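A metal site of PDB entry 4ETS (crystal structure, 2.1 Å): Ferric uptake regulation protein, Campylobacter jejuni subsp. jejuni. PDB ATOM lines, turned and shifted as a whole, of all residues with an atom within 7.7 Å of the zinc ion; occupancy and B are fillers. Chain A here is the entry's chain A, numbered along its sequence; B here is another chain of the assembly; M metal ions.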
ATOM      1  N   ILE A 109     -29.630 -28.428  12.836  1.00  0.00           N
ATOM      2  CA  ILE A 109     -28.457 -28.180  13.699  1.00  0.00           C
ATOM      3  C   ILE A 109     -28.531 -26.785  14.346  1.00  0.00           C
ATOM      4  O   ILE A 109     -28.682 -25.815  13.641  1.00  0.00           O
ATOM      5  CB  ILE A 109     -27.150 -28.303  12.837  1.00  0.00           C
ATOM      6  CG1 ILE A 109     -27.057 -29.719  12.281  1.00  0.00           C
ATOM      7  CG2 ILE A 109     -25.897 -27.928  13.640  1.00  0.00           C
ATOM      8  CD1 ILE A 109     -26.086 -29.937  11.153  1.00  0.00           C
ATOM      9  N   CYS A 110     -28.416 -26.691  15.677  1.00  0.00           N
ATOM     10  CA  CYS A 110     -28.365 -25.384  16.331  1.00  0.00           C
ATOM     11  C   CYS A 110     -26.940 -24.827  16.124  1.00  0.00           C
ATOM     12  O   CYS A 110     -26.021 -25.472  16.521  1.00  0.00           O
ATOM     13  CB  CYS A 110     -28.625 -25.440  17.858  1.00  0.00           C
ATOM     14  SG  CYS A 110     -28.407 -23.781  18.531  1.00  0.00           S
ATOM     15  N   LYS A 111     -26.834 -23.634  15.530  1.00  0.00           N
ATOM     16  CA  LYS A 111     -25.533 -22.959  15.203  1.00  0.00           C
ATOM     17  C   LYS A 111     -24.748 -22.609  16.513  1.00  0.00           C
ATOM     18  O   LYS A 111     -23.530 -22.467  16.499  1.00  0.00           O
ATOM     19  CB  LYS A 111     -25.782 -21.661  14.381  1.00  0.00           C
ATOM     20  CG  LYS A 111     -26.073 -21.926  12.877  1.00  0.00           C
ATOM     21  CD  LYS A 111     -26.219 -20.642  11.910  1.00  0.00           C
ATOM     22  CE  LYS A 111     -27.172 -21.025  10.669  1.00  0.00           C
ATOM     23  NZ  LYS A 111     -27.218 -20.336   9.219  1.00  0.00           N
ATOM     24  N   ASN A 112     -25.448 -22.512  17.615  1.00  0.00           N
ATOM     25  CA  ASN A 112     -24.785 -22.185  18.870  1.00  0.00           C
ATOM     26  C   ASN A 112     -24.332 -23.389  19.692  1.00  0.00           C
ATOM     27  O   ASN A 112     -23.140 -23.720  19.729  1.00  0.00           O
ATOM     28  CB  ASN A 112     -25.636 -21.242  19.710  1.00  0.00           C
ATOM     29  CG  ASN A 112     -24.858 -20.655  20.885  1.00  0.00           C
ATOM     30  OD1 ASN A 112     -23.861 -21.242  21.355  1.00  0.00           O
ATOM     31  ND2 ASN A 112     -25.328 -19.501  21.384  1.00  0.00           N
ATOM     32  N   CYS A 113     -25.266 -24.055  20.347  1.00  0.00           N
ATOM     33  CA  CYS A 113     -24.863 -25.153  21.230  1.00  0.00           C
ATOM     34  C   CYS A 113     -24.544 -26.437  20.503  1.00  0.00           C
ATOM     35  O   CYS A 113     -24.118 -27.373  21.136  1.00  0.00           O
ATOM     36  CB  CYS A 113     -25.992 -25.428  22.227  1.00  0.00           C
ATOM     37  SG  CYS A 113     -27.616 -25.957  21.451  1.00  0.00           S
ATOM     38  N   GLY A 114     -24.850 -26.538  19.197  1.00  0.00           N
ATOM     39  CA  GLY A 114     -24.609 -27.787  18.462  1.00  0.00           C
ATOM     40  C   GLY A 114     -25.607 -28.911  18.731  1.00  0.00           C
ATOM     41  O   GLY A 114     -25.354 -30.029  18.408  1.00  0.00           O
ATOM     42  N   LYS A 115     -26.733 -28.648  19.339  1.00  0.00           N
ATOM     43  CA  LYS A 115     -27.810 -29.651  19.449  1.00  0.00           C
ATOM     44  C   LYS A 115     -28.317 -30.049  18.028  1.00  0.00           C
ATOM     45  O   LYS A 115     -28.443 -29.188  17.148  1.00  0.00           O
ATOM     46  CB  LYS A 115     -28.946 -29.004  20.232  1.00  0.00           C
ATOM     47  CG  LYS A 115     -30.281 -29.641  20.028  1.00  0.00           C
ATOM     48  CD  LYS A 115     -31.347 -28.866  20.748  1.00  0.00           C
ATOM     49  CE  LYS A 115     -32.559 -29.754  21.014  1.00  0.00           C
ATOM     50  NZ  LYS A 115     -33.768 -28.905  21.285  1.00  0.00           N
ATOM     51  N   ILE A 116     -28.653 -31.334  17.834  1.00  0.00           N
ATOM     52  CA  ILE A 116     -29.033 -31.809  16.537  1.00  0.00           C
ATOM     53  C   ILE A 116     -30.383 -32.498  16.694  1.00  0.00           C
ATOM     54  O   ILE A 116     -30.595 -33.250  17.636  1.00  0.00           O
ATOM     55  CB  ILE A 116     -28.073 -32.808  15.946  1.00  0.00           C
ATOM     56  CG1 ILE A 116     -26.619 -32.282  15.921  1.00  0.00           C
ATOM     57  CG2 ILE A 116     -28.539 -33.301  14.554  1.00  0.00           C
ATOM     58  CD1 ILE A 116     -26.501 -30.884  15.617  1.00  0.00           C
ATOM     59  N   GLY A 148     -30.061 -23.400  12.289  1.00  0.00           N
ATOM     60  CA  GLY A 148     -30.826 -22.410  13.021  1.00  0.00           C
ATOM     61  C   GLY A 148     -30.313 -22.242  14.432  1.00  0.00           C
ATOM     62  O   GLY A 148     -29.174 -22.611  14.729  1.00  0.00           O
ATOM     63  N   VAL A 149     -31.133 -21.648  15.299  1.00  0.00           N
ATOM     64  CA  VAL A 149     -30.723 -21.457  16.678  1.00  0.00           C
ATOM     65  C   VAL A 149     -31.862 -22.022  17.502  1.00  0.00           C
ATOM     66  O   VAL A 149     -33.023 -21.691  17.285  1.00  0.00           O
ATOM     67  CB  VAL A 149     -30.454 -19.940  17.028  1.00  0.00           C
ATOM     68  CG1 VAL A 149     -30.196 -19.750  18.505  1.00  0.00           C
ATOM     69  CG2 VAL A 149     -29.220 -19.367  16.209  1.00  0.00           C
ATOM     70  N   CYS A 150     -31.533 -22.902  18.432  1.00  0.00           N
ATOM     71  CA  CYS A 150     -32.596 -23.513  19.236  1.00  0.00           C
ATOM     72  C   CYS A 150     -33.215 -22.501  20.203  1.00  0.00           C
ATOM     73  O   CYS A 150     -32.734 -21.342  20.331  1.00  0.00           O
ATOM     74  CB  CYS A 150     -32.078 -24.763  19.977  1.00  0.00           C
ATOM     75  SG  CYS A 150     -31.029 -24.364  21.408  1.00  0.00           S
ATOM     76  N   GLY A 151     -34.308 -22.950  20.848  1.00  0.00           N
ATOM     77  CA  GLY A 151     -35.080 -22.155  21.803  1.00  0.00           C
ATOM     78  C   GLY A 151     -34.226 -21.717  22.980  1.00  0.00           C
ATOM     79  O   GLY A 151     -34.269 -20.547  23.391  1.00  0.00           O
ATOM     80  N   ASP A 152     -33.423 -22.623  23.488  1.00  0.00           N
ATOM     81  CA  ASP A 152     -32.508 -22.282  24.576  1.00  0.00           C
ATOM     82  C   ASP A 152     -31.432 -21.258  24.168  1.00  0.00           C
ATOM     83  O   ASP A 152     -31.078 -20.401  24.977  1.00  0.00           O
ATOM     84  CB  ASP A 152     -31.839 -23.540  25.125  1.00  0.00           C
ATOM     85  CG  ASP A 152     -32.842 -24.529  25.674  1.00  0.00           C
ATOM     86  OD1 ASP A 152     -33.970 -24.125  26.004  1.00  0.00           O
ATOM     87  OD2 ASP A 152     -32.489 -25.723  25.805  1.00  0.00           O
ATOM     88  N   CYS A 153     -30.896 -21.348  22.959  1.00  0.00           N
ATOM     89  CA  CYS A 153     -29.869 -20.386  22.545  1.00  0.00           C
ATOM     90  C   CYS A 153     -30.446 -19.150  21.878  1.00  0.00           C
ATOM     91  O   CYS A 153     -29.680 -18.349  21.327  1.00  0.00           O
ATOM     92  CB  CYS A 153     -28.860 -21.021  21.580  1.00  0.00           C
ATOM     93  SG  CYS A 153     -27.993 -22.398  22.222  1.00  0.00           S
ATOM     94  N   ASN A 154     -31.777 -19.053  21.817  1.00  0.00           N
ATOM     95  CA  ASN A 154     -32.511 -17.917  21.257  1.00  0.00           C
ATOM     96  C   ASN A 154     -33.697 -18.120  20.326  1.00  0.00           C
ATOM     97  O   ASN A 154     -34.105 -17.160  19.652  1.00  0.00           O
ATOM     98  CB  ASN A 154     -31.563 -16.854  20.678  1.00  0.00           C
ATOM     99  CG  ASN A 154     -31.267 -15.776  21.676  1.00  0.00           C
ATOM    100  OD1 ASN A 154     -31.057 -16.096  22.855  1.00  0.00           O
ATOM    101  ND2 ASN A 154     -31.303 -14.483  21.253  1.00  0.00           N
ATOM    102  N   PHE B 137     -37.034 -23.965  17.133  1.00  0.00           N
ATOM    103  CA  PHE B 137     -35.857 -23.349  16.466  1.00  0.00           C
ATOM    104  C   PHE B 137     -36.279 -22.212  15.622  1.00  0.00           C
ATOM    105  O   PHE B 137     -37.412 -22.193  15.082  1.00  0.00           O
ATOM    106  CB  PHE B 137     -35.154 -24.288  15.468  1.00  0.00           C
ATOM    107  CG  PHE B 137     -34.138 -25.235  16.057  1.00  0.00           C
ATOM    108  CD1 PHE B 137     -34.508 -26.162  17.047  1.00  0.00           C
ATOM    109  CD2 PHE B 137     -32.837 -25.225  15.601  1.00  0.00           C
ATOM    110  CE1 PHE B 137     -33.572 -27.037  17.585  1.00  0.00           C
ATOM    111  CE2 PHE B 137     -31.878 -26.108  16.100  1.00  0.00           C
ATOM    112  CZ  PHE B 137     -32.223 -27.023  17.115  1.00  0.00           C
HETATM  113 ZN    ZN M   1     -28.829 -24.300  20.838  1.00  0.00          ZN
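N of Lys 115 lies close to SG of Cys 113 (3.5 Å).
The backbone NH of Asp 152 lies close to the side-chain sulfur of Cys 150 (3.6 Å).
SG of Cys 110 lies close to N of Asn 112 (3.3 Å).
The backbone NH (N) of Cys 110 lies within hydrogen-bond range of the backbone carbonyl oxygen (O) of Lys 115, at 2.9 Å.
The zinc ion is bound by SG of Cys 113 (2.1 Å), SG of Cys 150 (2.3 Å), SG of Cys 110 (2.4 Å) and SG of Cys 153 (2.5 Å).
The nearest printed residue that does not touch the zinc ion is Asn 112 (4.6 Å).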
